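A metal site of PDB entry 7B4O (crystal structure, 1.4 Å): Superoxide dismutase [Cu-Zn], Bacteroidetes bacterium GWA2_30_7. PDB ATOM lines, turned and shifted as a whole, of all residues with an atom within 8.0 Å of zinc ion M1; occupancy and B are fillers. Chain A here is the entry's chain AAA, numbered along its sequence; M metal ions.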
ATOM      1  N   PHE A  50      10.749   6.226 -30.333  1.00  0.00           N
ATOM      2  CA  PHE A  50      11.116   7.589 -30.782  1.00  0.00           C
ATOM      3  C   PHE A  50      10.980   8.497 -29.559  1.00  0.00           C
ATOM      4  O   PHE A  50       9.844   8.834 -29.177  1.00  0.00           O
ATOM      5  CB  PHE A  50      10.187   7.991 -31.934  1.00  0.00           C
ATOM      6  CG  PHE A  50      10.489   9.303 -32.598  1.00  0.00           C
ATOM      7  CD1 PHE A  50      11.550   9.441 -33.479  1.00  0.00           C
ATOM      8  CD2 PHE A  50       9.660  10.393 -32.380  1.00  0.00           C
ATOM      9  CE1 PHE A  50      11.801  10.660 -34.098  1.00  0.00           C
ATOM     10  CE2 PHE A  50       9.903  11.610 -33.005  1.00  0.00           C
ATOM     11  CZ  PHE A  50      10.973  11.744 -33.864  1.00  0.00           C
ATOM     12  N   HIS A  51      12.096   8.835 -28.909  1.00  0.00           N
ATOM     13  CA  HIS A  51      12.067   9.439 -27.562  1.00  0.00           C
ATOM     14  C   HIS A  51      13.019  10.616 -27.429  1.00  0.00           C
ATOM     15  O   HIS A  51      14.093  10.626 -28.055  1.00  0.00           O
ATOM     16  CB  HIS A  51      12.478   8.425 -26.499  1.00  0.00           C
ATOM     17  CG  HIS A  51      11.676   7.178 -26.488  1.00  0.00           C
ATOM     18  ND1 HIS A  51      12.273   5.971 -26.194  1.00  0.00           N
ATOM     19  CD2 HIS A  51      10.372   6.944 -26.735  1.00  0.00           C
ATOM     20  CE1 HIS A  51      11.345   5.032 -26.218  1.00  0.00           C
ATOM     21  NE2 HIS A  51      10.175   5.602 -26.574  1.00  0.00           N
ATOM     22  N   ILE A  52      12.634  11.546 -26.556  1.00  0.00           N
ATOM     23  CA  ILE A  52      13.584  12.558 -26.038  1.00  0.00           C
ATOM     24  C   ILE A  52      14.206  11.966 -24.781  1.00  0.00           C
ATOM     25  O   ILE A  52      13.431  11.589 -23.826  1.00  0.00           O
ATOM     26  CB  ILE A  52      12.910  13.909 -25.753  1.00  0.00           C
ATOM     27  CG1 ILE A  52      12.096  14.397 -26.948  1.00  0.00           C
ATOM     28  CG2 ILE A  52      13.939  14.916 -25.301  1.00  0.00           C
ATOM     29  CD1 ILE A  52      11.402  15.711 -26.724  1.00  0.00           C
ATOM     30  N   HIS A  53      15.524  11.850 -24.756  1.00  0.00           N
ATOM     31  CA  HIS A  53      16.272  11.366 -23.577  1.00  0.00           C
ATOM     32  C   HIS A  53      16.880  12.559 -22.847  1.00  0.00           C
ATOM     33  O   HIS A  53      16.931  13.663 -23.406  1.00  0.00           O
ATOM     34  CB  HIS A  53      17.266  10.280 -23.990  1.00  0.00           C
ATOM     35  CG  HIS A  53      16.651   8.938 -24.237  1.00  0.00           C
ATOM     36  ND1 HIS A  53      17.105   7.809 -23.603  1.00  0.00           N
ATOM     37  CD2 HIS A  53      15.655   8.533 -25.035  1.00  0.00           C
ATOM     38  CE1 HIS A  53      16.402   6.757 -23.995  1.00  0.00           C
ATOM     39  NE2 HIS A  53      15.533   7.154 -24.908  1.00  0.00           N
ATOM     40  N   GLY A  68      18.397   8.229 -19.545  1.00  0.00           N
ATOM     41  CA  GLY A  68      17.022   7.723 -19.600  1.00  0.00           C
ATOM     42  C   GLY A  68      16.082   8.705 -20.262  1.00  0.00           C
ATOM     43  O   GLY A  68      16.557   9.688 -20.860  1.00  0.00           O
ATOM     44  N   HIS A  69      14.784   8.446 -20.179  1.00  0.00           N
ATOM     45  CA  HIS A  69      13.763   9.308 -20.814  1.00  0.00           C
ATOM     46  C   HIS A  69      13.773  10.680 -20.154  1.00  0.00           C
ATOM     47  O   HIS A  69      13.955  10.774 -18.916  1.00  0.00           O
ATOM     48  CB  HIS A  69      12.382   8.646 -20.796  1.00  0.00           C
ATOM     49  CG  HIS A  69      12.344   7.481 -21.717  1.00  0.00           C
ATOM     50  ND1 HIS A  69      11.182   6.831 -22.062  1.00  0.00           N
ATOM     51  CD2 HIS A  69      13.340   6.903 -22.438  1.00  0.00           C
ATOM     52  CE1 HIS A  69      11.460   5.885 -22.942  1.00  0.00           C
ATOM     53  NE2 HIS A  69      12.786   5.895 -23.181  1.00  0.00           N
ATOM     54  N   PHE A  70      13.587  11.722 -20.953  1.00  0.00           N
ATOM     55  CA  PHE A  70      13.423  13.081 -20.397  1.00  0.00           C
ATOM     56  C   PHE A  70      12.103  13.105 -19.615  1.00  0.00           C
ATOM     57  O   PHE A  70      11.006  12.951 -20.200  1.00  0.00           O
ATOM     58  CB  PHE A  70      13.490  14.130 -21.503  1.00  0.00           C
ATOM     59  CG  PHE A  70      13.355  15.534 -21.013  1.00  0.00           C
ATOM     60  CD1 PHE A  70      14.128  15.990 -19.964  1.00  0.00           C
ATOM     61  CD2 PHE A  70      12.466  16.411 -21.608  1.00  0.00           C
ATOM     62  CE1 PHE A  70      14.024  17.300 -19.518  1.00  0.00           C
ATOM     63  CE2 PHE A  70      12.349  17.725 -21.147  1.00  0.00           C
ATOM     64  CZ  PHE A  70      13.127  18.156 -20.113  1.00  0.00           C
ATOM     65  N   ASN A  71      12.221  13.269 -18.302  1.00  0.00           N
ATOM     66  CA  ASN A  71      11.094  13.029 -17.371  1.00  0.00           C
ATOM     67  C   ASN A  71      11.149  14.037 -16.225  1.00  0.00           C
ATOM     68  O   ASN A  71      11.191  13.661 -15.057  1.00  0.00           O
ATOM     69  CB  ASN A  71      11.124  11.589 -16.874  1.00  0.00           C
ATOM     70  CG  ASN A  71       9.918  11.228 -16.035  1.00  0.00           C
ATOM     71  OD1 ASN A  71       8.856  11.852 -16.167  1.00  0.00           O
ATOM     72  ND2 ASN A  71      10.070  10.211 -15.218  1.00  0.00           N
ATOM     73  N   LYS A  75       7.083  11.253 -13.923  1.00  0.00           N
ATOM     74  CA  LYS A  75       5.866  10.489 -14.261  1.00  0.00           C
ATOM     75  C   LYS A  75       6.265   9.143 -14.874  1.00  0.00           C
ATOM     76  O   LYS A  75       7.467   8.874 -15.016  1.00  0.00           O
ATOM     77  CB  LYS A  75       4.967  11.357 -15.154  1.00  0.00           C
ATOM     78  CG  LYS A  75       4.290  12.477 -14.348  1.00  0.00           C
ATOM     79  CD  LYS A  75       3.360  13.374 -15.128  1.00  0.00           C
ATOM     80  CE  LYS A  75       2.161  12.660 -15.703  1.00  0.00           C
ATOM     81  NZ  LYS A  75       1.254  12.158 -14.656  1.00  0.00           N
ATOM     82  N   SER A  76       5.262   8.313 -15.135  1.00  0.00           N
ATOM     83  CA  SER A  76       5.416   6.958 -15.713  1.00  0.00           C
ATOM     84  C   SER A  76       5.575   7.072 -17.219  1.00  0.00           C
ATOM     85  O   SER A  76       5.171   8.065 -17.791  1.00  0.00           O
ATOM     86  CB  SER A  76       4.249   6.084 -15.355  1.00  0.00           C
ATOM     87  OG  SER A  76       4.172   5.923 -13.955  1.00  0.00           O
ATOM     88  N   HIS A  77       6.136   6.031 -17.836  1.00  0.00           N
ATOM     89  CA  HIS A  77       6.279   5.918 -19.300  1.00  0.00           C
ATOM     90  C   HIS A  77       4.895   5.682 -19.922  1.00  0.00           C
ATOM     91  O   HIS A  77       4.138   4.862 -19.377  1.00  0.00           O
ATOM     92  CB  HIS A  77       7.222   4.791 -19.667  1.00  0.00           C
ATOM     93  CG  HIS A  77       7.414   4.657 -21.138  1.00  0.00           C
ATOM     94  ND1 HIS A  77       8.150   5.564 -21.896  1.00  0.00           N
ATOM     95  CD2 HIS A  77       6.882   3.779 -22.014  1.00  0.00           C
ATOM     96  CE1 HIS A  77       8.088   5.199 -23.152  1.00  0.00           C
ATOM     97  NE2 HIS A  77       7.329   4.108 -23.262  1.00  0.00           N
ATOM     98  N   GLY A  78       4.600   6.320 -21.048  1.00  0.00           N
ATOM     99  CA  GLY A  78       3.361   6.050 -21.778  1.00  0.00           C
ATOM    100  C   GLY A  78       3.439   6.487 -23.232  1.00  0.00           C
ATOM    101  O   GLY A  78       4.559   6.675 -23.742  1.00  0.00           O
ATOM    102  N   ALA A  79       2.273   6.622 -23.852  1.00  0.00           N
ATOM    103  CA  ALA A  79       2.086   7.055 -25.249  1.00  0.00           C
ATOM    104  C   ALA A  79       1.989   8.575 -25.290  1.00  0.00           C
ATOM    105  O   ALA A  79       1.595   9.202 -24.310  1.00  0.00           O
ATOM    106  CB  ALA A  79       0.865   6.391 -25.828  1.00  0.00           C
ATOM    107  N   SER A  84      -0.452  10.142 -18.395  1.00  0.00           N
ATOM    108  CA  SER A  84       0.640   9.438 -17.685  1.00  0.00           C
ATOM    109  C   SER A  84       1.747   9.126 -18.697  1.00  0.00           C
ATOM    110  O   SER A  84       1.753   8.000 -19.257  1.00  0.00           O
ATOM    111  CB  SER A  84       0.120   8.221 -16.988  1.00  0.00           C
ATOM    112  OG  SER A  84       1.144   7.618 -16.240  1.00  0.00           O
ATOM    113  N   ARG A  85       2.618  10.091 -18.954  1.00  0.00           N
ATOM    114  CA  ARG A  85       3.753   9.965 -19.896  1.00  0.00           C
ATOM    115  C   ARG A  85       4.927  10.819 -19.416  1.00  0.00           C
ATOM    116  O   ARG A  85       4.728  11.781 -18.673  1.00  0.00           O
ATOM    117  CB  ARG A  85       3.344  10.365 -21.313  1.00  0.00           C
ATOM    118  CG  ARG A  85       2.972  11.835 -21.467  1.00  0.00           C
ATOM    119  CD  ARG A  85       2.850  12.244 -22.923  1.00  0.00           C
ATOM    120  NE  ARG A  85       4.096  12.839 -23.440  1.00  0.00           N
ATOM    121  CZ  ARG A  85       4.167  13.607 -24.513  1.00  0.00           C
ATOM    122  NH1 ARG A  85       3.091  13.853 -25.232  1.00  0.00           N
ATOM    123  NH2 ARG A  85       5.331  14.133 -24.856  1.00  0.00           N
ATOM    124  N   HIS A  86       6.111  10.451 -19.883  1.00  0.00           N
ATOM    125  CA  HIS A  86       7.323  11.298 -19.810  1.00  0.00           C
ATOM    126  C   HIS A  86       7.183  12.400 -20.851  1.00  0.00           C
ATOM    127  O   HIS A  86       6.566  12.156 -21.901  1.00  0.00           O
ATOM    128  CB  HIS A  86       8.568  10.446 -20.120  1.00  0.00           C
ATOM    129  CG  HIS A  86       8.767   9.292 -19.204  1.00  0.00           C
ATOM    130  ND1 HIS A  86       9.285   8.097 -19.619  1.00  0.00           N
ATOM    131  CD2 HIS A  86       8.503   9.163 -17.889  1.00  0.00           C
ATOM    132  CE1 HIS A  86       9.366   7.293 -18.581  1.00  0.00           C
ATOM    133  NE2 HIS A  86       8.895   7.909 -17.517  1.00  0.00           N
ATOM    134  N   ILE A  87       7.730  13.580 -20.582  1.00  0.00           N
ATOM    135  CA  ILE A  87       7.818  14.638 -21.619  1.00  0.00           C
ATOM    136  C   ILE A  87       8.440  14.017 -22.873  1.00  0.00           C
ATOM    137  O   ILE A  87       7.963  14.300 -23.987  1.00  0.00           O
ATOM    138  CB  ILE A  87       8.594  15.865 -21.128  1.00  0.00           C
ATOM    139  CG1 ILE A  87       7.921  16.558 -19.947  1.00  0.00           C
ATOM    140  CG2 ILE A  87       8.812  16.833 -22.286  1.00  0.00           C
ATOM    141  CD1 ILE A  87       6.482  16.968 -20.174  1.00  0.00           C
ATOM    142  N   GLY A  88       9.428  13.151 -22.705  1.00  0.00           N
ATOM    143  CA  GLY A  88      10.167  12.582 -23.860  1.00  0.00           C
ATOM    144  C   GLY A  88       9.437  11.476 -24.595  1.00  0.00           C
ATOM    145  O   GLY A  88      10.041  10.910 -25.531  1.00  0.00           O
ATOM    146  N   ASP A  89       8.211  11.102 -24.222  1.00  0.00           N
ATOM    147  CA  ASP A  89       7.502   9.952 -24.821  1.00  0.00           C
ATOM    148  C   ASP A  89       6.807  10.353 -26.122  1.00  0.00           C
ATOM    149  O   ASP A  89       5.621  10.696 -26.090  1.00  0.00           O
ATOM    150  CB  ASP A  89       6.534   9.321 -23.821  1.00  0.00           C
ATOM    151  CG  ASP A  89       7.264   8.604 -22.695  1.00  0.00           C
ATOM    152  OD1 ASP A  89       8.496   8.372 -22.821  1.00  0.00           O
ATOM    153  OD2 ASP A  89       6.586   8.296 -21.688  1.00  0.00           O
ATOM    154  N   LEU A  90       7.546  10.323 -27.234  1.00  0.00           N
ATOM    155  CA  LEU A  90       7.012  10.723 -28.558  1.00  0.00           C
ATOM    156  C   LEU A  90       6.582   9.487 -29.354  1.00  0.00           C
ATOM    157  O   LEU A  90       6.297   9.633 -30.537  1.00  0.00           O
ATOM    158  CB  LEU A  90       8.045  11.554 -29.325  1.00  0.00           C
ATOM    159  CG  LEU A  90       8.735  12.686 -28.564  1.00  0.00           C
ATOM    160  CD1 LEU A  90       9.493  13.570 -29.524  1.00  0.00           C
ATOM    161  CD2 LEU A  90       7.762  13.541 -27.744  1.00  0.00           C
ATOM    162  N   GLY A  91       6.448   8.322 -28.703  1.00  0.00           N
ATOM    163  CA  GLY A  91       5.820   7.120 -29.274  1.00  0.00           C
ATOM    164  C   GLY A  91       6.751   6.374 -30.223  1.00  0.00           C
ATOM    165  O   GLY A  91       7.894   6.071 -29.835  1.00  0.00           O
ATOM    166  N   ASP A 130       8.337   0.804 -29.240  1.00  0.00           N
ATOM    167  CA  ASP A 130       7.941   1.195 -27.871  1.00  0.00           C
ATOM    168  C   ASP A 130       6.539   0.630 -27.641  1.00  0.00           C
ATOM    169  O   ASP A 130       5.629   1.030 -28.389  1.00  0.00           O
ATOM    170  CB  ASP A 130       7.994   2.720 -27.758  1.00  0.00           C
ATOM    171  CG  ASP A 130       7.565   3.307 -26.425  1.00  0.00           C
ATOM    172  OD1 ASP A 130       6.971   2.591 -25.594  1.00  0.00           O
ATOM    173  OD2 ASP A 130       7.806   4.507 -26.234  1.00  0.00           O
ATOM    174  N   THR A 134       5.226  -0.839 -20.916  1.00  0.00           N
ATOM    175  CA  THR A 134       6.257  -1.436 -20.030  1.00  0.00           C
ATOM    176  C   THR A 134       7.057  -0.289 -19.379  1.00  0.00           C
ATOM    177  O   THR A 134       7.496   0.612 -20.121  1.00  0.00           O
ATOM    178  CB  THR A 134       7.155  -2.424 -20.761  1.00  0.00           C
ATOM    179  OG1 THR A 134       6.341  -3.437 -21.337  1.00  0.00           O
ATOM    180  CG2 THR A 134       8.176  -3.061 -19.834  1.00  0.00           C
ATOM    181  N   GLN A 135       7.220  -0.338 -18.056  1.00  0.00           N
ATOM    182  CA  GLN A 135       7.975   0.672 -17.290  1.00  0.00           C
ATOM    183  C   GLN A 135       9.423   0.218 -17.192  1.00  0.00           C
ATOM    184  O   GLN A 135       9.676  -0.985 -17.070  1.00  0.00           O
ATOM    185  CB  GLN A 135       7.347   0.871 -15.911  1.00  0.00           C
ATOM    186  CG  GLN A 135       5.894   1.312 -15.983  1.00  0.00           C
ATOM    187  CD  GLN A 135       5.740   2.606 -16.736  1.00  0.00           C
ATOM    188  OE1 GLN A 135       6.417   3.586 -16.454  1.00  0.00           O
ATOM    189  NE2 GLN A 135       4.845   2.612 -17.709  1.00  0.00           N
ATOM    190  N   PRO A 136      10.412   1.138 -17.206  1.00  0.00           N
ATOM    191  CA  PRO A 136      10.177   2.565 -17.420  1.00  0.00           C
ATOM    192  C   PRO A 136      10.434   3.120 -18.844  1.00  0.00           C
ATOM    193  O   PRO A 136      10.389   4.326 -19.016  1.00  0.00           O
ATOM    194  CB  PRO A 136      11.229   3.168 -16.476  1.00  0.00           C
ATOM    195  CG  PRO A 136      12.414   2.225 -16.615  1.00  0.00           C
ATOM    196  CD  PRO A 136      11.801   0.858 -16.840  1.00  0.00           C
ATOM    197  N   THR A 137      10.680   2.250 -19.823  1.00  0.00           N
ATOM    198  CA  THR A 137      11.159   2.666 -21.171  1.00  0.00           C
ATOM    199  C   THR A 137      10.290   2.166 -22.332  1.00  0.00           C
ATOM    200  O   THR A 137      10.616   2.568 -23.448  1.00  0.00           O
ATOM    201  CB  THR A 137      12.609   2.214 -21.406  1.00  0.00           C
ATOM    202  OG1 THR A 137      12.602   0.812 -21.683  1.00  0.00           O
ATOM    203  CG2 THR A 137      13.510   2.471 -20.226  1.00  0.00           C
ATOM    204  N   GLY A 138       9.265   1.330 -22.117  1.00  0.00           N
ATOM    205  CA  GLY A 138       8.478   0.760 -23.244  1.00  0.00           C
ATOM    206  C   GLY A 138       9.171  -0.388 -23.963  1.00  0.00           C
ATOM    207  O   GLY A 138       8.648  -0.833 -25.004  1.00  0.00           O
HETATM  208 ZN    ZN M   1       9.245   7.256 -21.447  1.00  0.00          ZN
HETATM  209 ZN    ZN M   2      14.208   5.705 -25.423  1.00  0.00          ZN
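Residues that only touch zinc ion M1: Pro 136 (3.98 Å).
Five residues have an atom within 4 Å of zinc ion M1: His 69, His 77, His 86, Asp 89 and Pro 136.
The side-chain carboxylate (OD2) of Asp 89 is in hydrogen-bond range of the backbone NH (N) of Gly 78 (2.9 Å).
N of His 86 is in hydrogen-bond range of O of Ser 76, at 3.3 Å.
A ring nitrogen (NE2) of His 86 sits close to the side-chain amide nitrogen (ND2) of Asn 71 (3.5 Å).
A ring nitrogen (NE2) of His 86 sits at hydrogen-bond distance from the backbone carbonyl oxygen (O) of Lys 75 (3.0 Å).
NE2 of His 77 is in hydrogen-bond range of OD1 of Asp 130 (2.8 Å).
N of His 77 lies within hydrogen-bond range of OE1 of Gln 135 (2.8 Å).
A ring nitrogen (NE2) of His 69 sits close to a ring nitrogen (ND1) of His 51.
A ring nitrogen (NE2) of His 69 lies close to a ring nitrogen (NE2) of His 53 (3.5 Å).
Zinc ion M1 is bound by the side-chain carboxylate (OD1) of Asp 89, a ring nitrogen (ND1) of His 86, a ring nitrogen (ND1) of His 77 and a ring nitrogen (ND1) of His 69.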
